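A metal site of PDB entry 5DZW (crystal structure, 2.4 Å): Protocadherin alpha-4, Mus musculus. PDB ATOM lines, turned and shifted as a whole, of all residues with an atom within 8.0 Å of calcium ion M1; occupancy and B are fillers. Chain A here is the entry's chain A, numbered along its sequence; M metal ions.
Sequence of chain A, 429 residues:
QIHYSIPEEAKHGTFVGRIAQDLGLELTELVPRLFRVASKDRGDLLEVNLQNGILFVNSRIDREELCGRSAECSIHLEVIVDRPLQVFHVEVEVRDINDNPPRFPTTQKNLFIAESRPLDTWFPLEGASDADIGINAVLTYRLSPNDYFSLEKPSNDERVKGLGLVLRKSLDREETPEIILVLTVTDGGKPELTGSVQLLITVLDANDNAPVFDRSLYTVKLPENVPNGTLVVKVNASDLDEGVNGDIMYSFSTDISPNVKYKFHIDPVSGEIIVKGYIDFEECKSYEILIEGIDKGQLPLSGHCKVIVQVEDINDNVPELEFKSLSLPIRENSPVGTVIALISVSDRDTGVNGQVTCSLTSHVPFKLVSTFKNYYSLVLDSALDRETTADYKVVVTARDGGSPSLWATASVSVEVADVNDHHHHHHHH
The side-chain amide nitrogen (ND2) of Asn 98 sits at hydrogen-bond distance from the backbone carbonyl oxygen (O) of Gly 189 (2.5 Å). The side-chain carboxylate (OD2) of Asp 132 is in hydrogen-bond range of the backbone NH (N) of Asp 99 (3.4 Å). OD2 of Asp 187 is in hydrogen-bond range of ND2 of Asn 98. The side-chain carboxylate (OD1) of Asp 187 is in hydrogen-bond range of the backbone NH (N) of Leu 193 (2.8 Å). The side-chain amide nitrogen (ND2) of Asn 136 is in hydrogen-bond range of the side-chain carboxylate (OD1) of Asp 96 (2.7 Å). The backbone carbonyl oxygen (O) of Pro 191 lies within hydrogen-bond range of the side-chain amide nitrogen (ND2) of Asn 98. The side-chain carboxylate (OE2) of Glu 64 lies close to the side-chain amide nitrogen (ND2) of Asn 100 (3.1 Å). OD2 of Asp 132 sits close to OD1 of Asn 98, 3.2 Å away.
Residues that only touch calcium ion M1: Asp 187 (3.6 Å). Of the 27 residues printed, 6 come within 4 Å of calcium ion M1.
Calcium ion M1 is bound by the backbone carbonyl oxygen of Asn 100 (2.5 Å), the side-chain amide oxygen of Asn 98 (2.5 Å), the side-chain carboxylate of Asp 130 (2.5 Å) and the backbone carbonyl oxygen of Asn 136 (2.7 Å). Calcium ion M1 has four donor atoms within binding distance. Slightly farther from calcium ion M1 lies the side-chain carboxylate (OD2) of Asp 132 (3.0 Å). Slightly farther from calcium ion M1 lies OD1 of Asp 130 (3.1 Å).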
ATOM      1  N   GLU A  64     -16.109 -20.344  -5.179  1.00  0.00           N
ATOM      2  CA  GLU A  64     -14.753 -20.340  -4.633  1.00  0.00           C
ATOM      3  C   GLU A  64     -14.735 -20.045  -3.139  1.00  0.00           C
ATOM      4  O   GLU A  64     -13.757 -20.334  -2.454  1.00  0.00           O
ATOM      5  CB  GLU A  64     -13.888 -19.309  -5.373  1.00  0.00           C
ATOM      6  CG  GLU A  64     -13.785 -19.524  -6.879  1.00  0.00           C
ATOM      7  CD  GLU A  64     -14.919 -18.883  -7.643  1.00  0.00           C
ATOM      8  OE1 GLU A  64     -16.091 -19.061  -7.248  1.00  0.00           O
ATOM      9  OE2 GLU A  64     -14.641 -18.189  -8.641  1.00  0.00           O
ATOM     10  N   ASP A  96     -18.578 -24.521 -11.969  1.00  0.00           N
ATOM     11  CA  ASP A  96     -17.660 -23.388 -11.969  1.00  0.00           C
ATOM     12  C   ASP A  96     -17.920 -22.425 -13.121  1.00  0.00           C
ATOM     13  O   ASP A  96     -18.186 -22.830 -14.242  1.00  0.00           O
ATOM     14  CB  ASP A  96     -16.214 -23.884 -12.024  1.00  0.00           C
ATOM     15  CG  ASP A  96     -15.195 -22.764 -11.970  1.00  0.00           C
ATOM     16  OD1 ASP A  96     -14.216 -22.806 -12.745  1.00  0.00           O
ATOM     17  OD2 ASP A  96     -15.378 -21.829 -11.156  1.00  0.00           O
ATOM     18  N   ILE A  97     -17.847 -21.129 -12.812  1.00  0.00           N
ATOM     19  CA  ILE A  97     -17.940 -20.082 -13.826  1.00  0.00           C
ATOM     20  C   ILE A  97     -16.653 -19.277 -13.872  1.00  0.00           C
ATOM     21  O   ILE A  97     -16.159 -18.822 -12.832  1.00  0.00           O
ATOM     22  CB  ILE A  97     -19.133 -19.147 -13.559  1.00  0.00           C
ATOM     23  CG1 ILE A  97     -20.450 -19.850 -13.871  1.00  0.00           C
ATOM     24  CG2 ILE A  97     -19.019 -17.867 -14.384  1.00  0.00           C
ATOM     25  CD1 ILE A  97     -21.653 -18.931 -13.886  1.00  0.00           C
ATOM     26  N   ASN A  98     -16.103 -19.100 -15.069  1.00  0.00           N
ATOM     27  CA  ASN A  98     -14.859 -18.352 -15.237  1.00  0.00           C
ATOM     28  C   ASN A  98     -15.056 -16.860 -14.986  1.00  0.00           C
ATOM     29  O   ASN A  98     -15.057 -16.061 -15.915  1.00  0.00           O
ATOM     30  CB  ASN A  98     -14.285 -18.568 -16.644  1.00  0.00           C
ATOM     31  CG  ASN A  98     -12.839 -18.128 -16.767  1.00  0.00           C
ATOM     32  OD1 ASN A  98     -12.159 -17.920 -15.763  1.00  0.00           O
ATOM     33  ND2 ASN A  98     -12.367 -17.990 -17.999  1.00  0.00           N
ATOM     34  N   ASP A  99     -15.238 -16.496 -13.721  1.00  0.00           N
ATOM     35  CA  ASP A  99     -15.495 -15.103 -13.361  1.00  0.00           C
ATOM     36  C   ASP A  99     -14.324 -14.474 -12.616  1.00  0.00           C
ATOM     37  O   ASP A  99     -14.428 -13.373 -12.076  1.00  0.00           O
ATOM     38  CB  ASP A  99     -16.776 -14.983 -12.525  1.00  0.00           C
ATOM     39  CG  ASP A  99     -16.682 -15.721 -11.196  1.00  0.00           C
ATOM     40  OD1 ASP A  99     -15.900 -16.686 -11.096  1.00  0.00           O
ATOM     41  OD2 ASP A  99     -17.404 -15.326 -10.248  1.00  0.00           O
ATOM     42  N   ASN A 100     -13.195 -15.188 -12.580  1.00  0.00           N
ATOM     43  CA  ASN A 100     -11.965 -14.656 -11.992  1.00  0.00           C
ATOM     44  C   ASN A 100     -10.784 -14.749 -12.951  1.00  0.00           C
ATOM     45  O   ASN A 100     -10.512 -15.812 -13.501  1.00  0.00           O
ATOM     46  CB  ASN A 100     -11.647 -15.384 -10.689  1.00  0.00           C
ATOM     47  CG  ASN A 100     -12.547 -14.980  -9.549  1.00  0.00           C
ATOM     48  OD1 ASN A 100     -13.148 -13.908  -9.566  1.00  0.00           O
ATOM     49  ND2 ASN A 100     -12.651 -15.840  -8.544  1.00  0.00           N
ATOM     50  N   PRO A 101     -10.078 -13.630 -13.142  1.00  0.00           N
ATOM     51  CA  PRO A 101      -8.923 -13.553 -14.039  1.00  0.00           C
ATOM     52  C   PRO A 101      -7.637 -14.079 -13.401  1.00  0.00           C
ATOM     53  O   PRO A 101      -7.515 -14.058 -12.182  1.00  0.00           O
ATOM     54  CB  PRO A 101      -8.800 -12.053 -14.321  1.00  0.00           C
ATOM     55  CG  PRO A 101      -9.289 -11.424 -13.060  1.00  0.00           C
ATOM     56  CD  PRO A 101     -10.385 -12.321 -12.540  1.00  0.00           C
ATOM     57  N   PRO A 102      -6.689 -14.546 -14.234  1.00  0.00           N
ATOM     58  CA  PRO A 102      -5.362 -14.942 -13.742  1.00  0.00           C
ATOM     59  C   PRO A 102      -4.613 -13.745 -13.162  1.00  0.00           C
ATOM     60  O   PRO A 102      -4.396 -12.762 -13.878  1.00  0.00           O
ATOM     61  CB  PRO A 102      -4.664 -15.482 -14.995  1.00  0.00           C
ATOM     62  CG  PRO A 102      -5.763 -15.809 -15.946  1.00  0.00           C
ATOM     63  CD  PRO A 102      -6.834 -14.801 -15.666  1.00  0.00           C
ATOM     64  N   ARG A 103      -4.229 -13.820 -11.891  1.00  0.00           N
ATOM     65  CA  ARG A 103      -3.575 -12.701 -11.232  1.00  0.00           C
ATOM     66  C   ARG A 103      -2.141 -13.033 -10.807  1.00  0.00           C
ATOM     67  O   ARG A 103      -1.874 -14.103 -10.280  1.00  0.00           O
ATOM     68  CB  ARG A 103      -4.382 -12.253 -10.011  1.00  0.00           C
ATOM     69  N   SER A 129      -1.589 -17.057 -10.270  1.00  0.00           N
ATOM     70  CA  SER A 129      -2.521 -17.963  -9.594  1.00  0.00           C
ATOM     71  C   SER A 129      -3.940 -17.684 -10.049  1.00  0.00           C
ATOM     72  O   SER A 129      -4.249 -16.584 -10.522  1.00  0.00           O
ATOM     73  CB  SER A 129      -2.413 -17.821  -8.075  1.00  0.00           C
ATOM     74  OG  SER A 129      -2.816 -16.539  -7.656  1.00  0.00           O
ATOM     75  N   ASP A 130      -4.809 -18.676  -9.922  1.00  0.00           N
ATOM     76  CA  ASP A 130      -6.206 -18.526 -10.311  1.00  0.00           C
ATOM     77  C   ASP A 130      -7.124 -19.154  -9.272  1.00  0.00           C
ATOM     78  O   ASP A 130      -6.854 -20.250  -8.770  1.00  0.00           O
ATOM     79  CB  ASP A 130      -6.455 -19.136 -11.685  1.00  0.00           C
ATOM     80  CG  ASP A 130      -7.740 -18.656 -12.321  1.00  0.00           C
ATOM     81  OD1 ASP A 130      -8.038 -17.444 -12.207  1.00  0.00           O
ATOM     82  OD2 ASP A 130      -8.457 -19.486 -12.913  1.00  0.00           O
ATOM     83  N   ALA A 131      -8.203 -18.458  -8.939  1.00  0.00           N
ATOM     84  CA  ALA A 131      -9.143 -18.929  -7.932  1.00  0.00           C
ATOM     85  C   ALA A 131     -10.038 -20.042  -8.469  1.00  0.00           C
ATOM     86  O   ALA A 131     -10.485 -20.911  -7.731  1.00  0.00           O
ATOM     87  CB  ALA A 131      -9.989 -17.774  -7.409  1.00  0.00           C
ATOM     88  N   ASP A 132     -10.290 -20.001  -9.783  1.00  0.00           N
ATOM     89  CA  ASP A 132     -11.157 -20.973 -10.424  1.00  0.00           C
ATOM     90  C   ASP A 132     -10.472 -22.334 -10.544  1.00  0.00           C
ATOM     91  O   ASP A 132      -9.265 -22.450 -10.344  1.00  0.00           O
ATOM     92  CB  ASP A 132     -11.580 -20.470 -11.804  1.00  0.00           C
ATOM     93  CG  ASP A 132     -12.333 -19.158 -11.738  1.00  0.00           C
ATOM     94  OD1 ASP A 132     -12.314 -18.518 -10.659  1.00  0.00           O
ATOM     95  OD2 ASP A 132     -12.928 -18.756 -12.755  1.00  0.00           O
ATOM     96  N   ILE A 133     -11.255 -23.359 -10.868  1.00  0.00           N
ATOM     97  CA  ILE A 133     -10.742 -24.715 -10.990  1.00  0.00           C
ATOM     98  C   ILE A 133     -11.247 -25.378 -12.265  1.00  0.00           C
ATOM     99  O   ILE A 133     -12.439 -25.306 -12.573  1.00  0.00           O
ATOM    100  CB  ILE A 133     -11.125 -25.587  -9.773  1.00  0.00           C
ATOM    101  CG1 ILE A 133     -10.531 -25.009  -8.473  1.00  0.00           C
ATOM    102  CG2 ILE A 133     -10.646 -27.021  -9.960  1.00  0.00           C
ATOM    103  CD1 ILE A 133      -9.018 -25.029  -8.431  1.00  0.00           C
ATOM    104  N   GLY A 134     -10.346 -26.021 -12.999  1.00  0.00           N
ATOM    105  CA  GLY A 134     -10.711 -26.720 -14.211  1.00  0.00           C
ATOM    106  C   GLY A 134     -10.119 -26.081 -15.452  1.00  0.00           C
ATOM    107  O   GLY A 134      -8.975 -25.619 -15.433  1.00  0.00           O
ATOM    108  N   ILE A 135     -10.890 -26.061 -16.536  1.00  0.00           N
ATOM    109  CA  ILE A 135     -10.458 -25.432 -17.767  1.00  0.00           C
ATOM    110  C   ILE A 135     -10.340 -23.916 -17.568  1.00  0.00           C
ATOM    111  O   ILE A 135      -9.515 -23.253 -18.198  1.00  0.00           O
ATOM    112  CB  ILE A 135     -11.430 -25.730 -18.929  1.00  0.00           C
ATOM    113  CG1 ILE A 135     -11.633 -27.239 -19.066  1.00  0.00           C
ATOM    114  CG2 ILE A 135     -10.920 -25.150 -20.240  1.00  0.00           C
ATOM    115  CD1 ILE A 135     -12.526 -27.643 -20.227  1.00  0.00           C
ATOM    116  N   ASN A 136     -11.155 -23.394 -16.657  1.00  0.00           N
ATOM    117  CA  ASN A 136     -11.105 -21.975 -16.305  1.00  0.00           C
ATOM    118  C   ASN A 136      -9.813 -21.618 -15.582  1.00  0.00           C
ATOM    119  O   ASN A 136      -9.488 -20.444 -15.428  1.00  0.00           O
ATOM    120  CB  ASN A 136     -12.310 -21.596 -15.448  1.00  0.00           C
ATOM    121  CG  ASN A 136     -13.634 -21.949 -16.100  1.00  0.00           C
ATOM    122  OD1 ASN A 136     -13.724 -22.056 -17.323  1.00  0.00           O
ATOM    123  ND2 ASN A 136     -14.671 -22.132 -15.285  1.00  0.00           N
ATOM    124  N   ALA A 137      -9.088 -22.643 -15.138  1.00  0.00           N
ATOM    125  CA  ALA A 137      -7.836 -22.438 -14.413  1.00  0.00           C
ATOM    126  C   ALA A 137      -6.623 -22.789 -15.270  1.00  0.00           C
ATOM    127  O   ALA A 137      -5.492 -22.530 -14.864  1.00  0.00           O
ATOM    128  CB  ALA A 137      -7.836 -23.263 -13.132  1.00  0.00           C
ATOM    129  N   VAL A 138      -6.868 -23.375 -16.428  1.00  0.00           N
ATOM    130  CA  VAL A 138      -5.782 -23.717 -17.353  1.00  0.00           C
ATOM    131  C   VAL A 138      -5.144 -22.450 -17.905  1.00  0.00           C
ATOM    132  O   VAL A 138      -5.766 -21.707 -18.665  1.00  0.00           O
ATOM    133  CB  VAL A 138      -6.278 -24.592 -18.522  1.00  0.00           C
ATOM    134  CG1 VAL A 138      -5.162 -24.801 -19.528  1.00  0.00           C
ATOM    135  CG2 VAL A 138      -6.783 -25.926 -17.994  1.00  0.00           C
ATOM    136  N   LEU A 139      -3.893 -22.205 -17.514  1.00  0.00           N
ATOM    137  CA  LEU A 139      -3.218 -20.951 -17.845  1.00  0.00           C
ATOM    138  C   LEU A 139      -2.346 -21.060 -19.089  1.00  0.00           C
ATOM    139  O   LEU A 139      -1.609 -22.036 -19.264  1.00  0.00           O
ATOM    140  CB  LEU A 139      -2.378 -20.492 -16.656  1.00  0.00           C
ATOM    141  CG  LEU A 139      -3.135 -20.258 -15.349  1.00  0.00           C
ATOM    142  CD1 LEU A 139      -2.174 -20.015 -14.199  1.00  0.00           C
ATOM    143  CD2 LEU A 139      -4.092 -19.088 -15.501  1.00  0.00           C
ATOM    144  N   THR A 186      -3.547 -15.865 -20.316  1.00  0.00           N
ATOM    145  CA  THR A 186      -4.969 -16.049 -20.577  1.00  0.00           C
ATOM    146  C   THR A 186      -5.448 -17.427 -20.127  1.00  0.00           C
ATOM    147  O   THR A 186      -4.797 -18.436 -20.410  1.00  0.00           O
ATOM    148  CB  THR A 186      -5.309 -15.866 -22.073  1.00  0.00           C
ATOM    149  OG1 THR A 186      -4.688 -16.911 -22.832  1.00  0.00           O
ATOM    150  CG2 THR A 186      -4.810 -14.520 -22.572  1.00  0.00           C
ATOM    151  N   ASP A 187      -6.580 -17.476 -19.437  1.00  0.00           N
ATOM    152  CA  ASP A 187      -7.147 -18.746 -19.009  1.00  0.00           C
ATOM    153  C   ASP A 187      -7.761 -19.482 -20.202  1.00  0.00           C
ATOM    154  O   ASP A 187      -7.998 -18.900 -21.254  1.00  0.00           O
ATOM    155  CB  ASP A 187      -8.211 -18.528 -17.922  1.00  0.00           C
ATOM    156  CG  ASP A 187      -9.111 -17.346 -18.210  1.00  0.00           C
ATOM    157  OD1 ASP A 187      -9.388 -17.066 -19.397  1.00  0.00           O
ATOM    158  OD2 ASP A 187      -9.552 -16.689 -17.239  1.00  0.00           O
ATOM    159  N   GLY A 188      -8.008 -20.780 -20.027  1.00  0.00           N
ATOM    160  CA  GLY A 188      -8.515 -21.612 -21.110  1.00  0.00           C
ATOM    161  C   GLY A 188     -10.021 -21.601 -21.237  1.00  0.00           C
ATOM    162  O   GLY A 188     -10.569 -21.938 -22.288  1.00  0.00           O
ATOM    163  N   GLY A 189     -10.711 -21.214 -20.165  1.00  0.00           N
ATOM    164  CA  GLY A 189     -12.164 -21.188 -20.170  1.00  0.00           C
ATOM    165  C   GLY A 189     -12.725 -19.897 -20.724  1.00  0.00           C
ATOM    166  O   GLY A 189     -12.246 -18.816 -20.397  1.00  0.00           O
ATOM    167  N   PRO A 191     -15.678 -17.044 -21.036  1.00  0.00           N
ATOM    168  CA  PRO A 191     -14.907 -15.986 -21.708  1.00  0.00           C
ATOM    169  C   PRO A 191     -13.479 -15.862 -21.184  1.00  0.00           C
ATOM    170  O   PRO A 191     -13.212 -16.187 -20.023  1.00  0.00           O
ATOM    171  CB  PRO A 191     -15.704 -14.718 -21.392  1.00  0.00           C
ATOM    172  CG  PRO A 191     -16.341 -15.010 -20.084  1.00  0.00           C
ATOM    173  CD  PRO A 191     -16.679 -16.476 -20.114  1.00  0.00           C
ATOM    174  N   GLU A 192     -12.573 -15.386 -22.034  1.00  0.00           N
ATOM    175  CA  GLU A 192     -11.163 -15.302 -21.697  1.00  0.00           C
ATOM    176  C   GLU A 192     -10.864 -14.126 -20.774  1.00  0.00           C
ATOM    177  O   GLU A 192     -11.335 -13.012 -21.007  1.00  0.00           O
ATOM    178  CB  GLU A 192     -10.317 -15.197 -22.967  1.00  0.00           C
ATOM    179  CG  GLU A 192     -10.828 -16.022 -24.137  1.00  0.00           C
ATOM    180  CD  GLU A 192     -10.682 -17.516 -23.924  1.00  0.00           C
ATOM    181  OE1 GLU A 192      -9.891 -17.920 -23.051  1.00  0.00           O
ATOM    182  OE2 GLU A 192     -11.367 -18.287 -24.627  1.00  0.00           O
ATOM    183  N   LEU A 193     -10.088 -14.371 -19.731  1.00  0.00           N
ATOM    184  CA  LEU A 193      -9.613 -13.300 -18.863  1.00  0.00           C
ATOM    185  C   LEU A 193      -8.087 -13.251 -18.877  1.00  0.00           C
ATOM    186  O   LEU A 193      -7.429 -14.283 -18.962  1.00  0.00           O
ATOM    187  CB  LEU A 193     -10.143 -13.475 -17.435  1.00  0.00           C
ATOM    188  CG  LEU A 193     -11.655 -13.325 -17.249  1.00  0.00           C
ATOM    189  CD1 LEU A 193     -12.344 -14.674 -17.314  1.00  0.00           C
ATOM    190  CD2 LEU A 193     -11.975 -12.613 -15.937  1.00  0.00           C
HETATM  191 CA    CA M   1     -10.337 -18.245 -14.072  1.00  0.00          CA
HETATM  192 CA    CA M   2     -15.311 -19.561 -10.529  1.00  0.00          CA
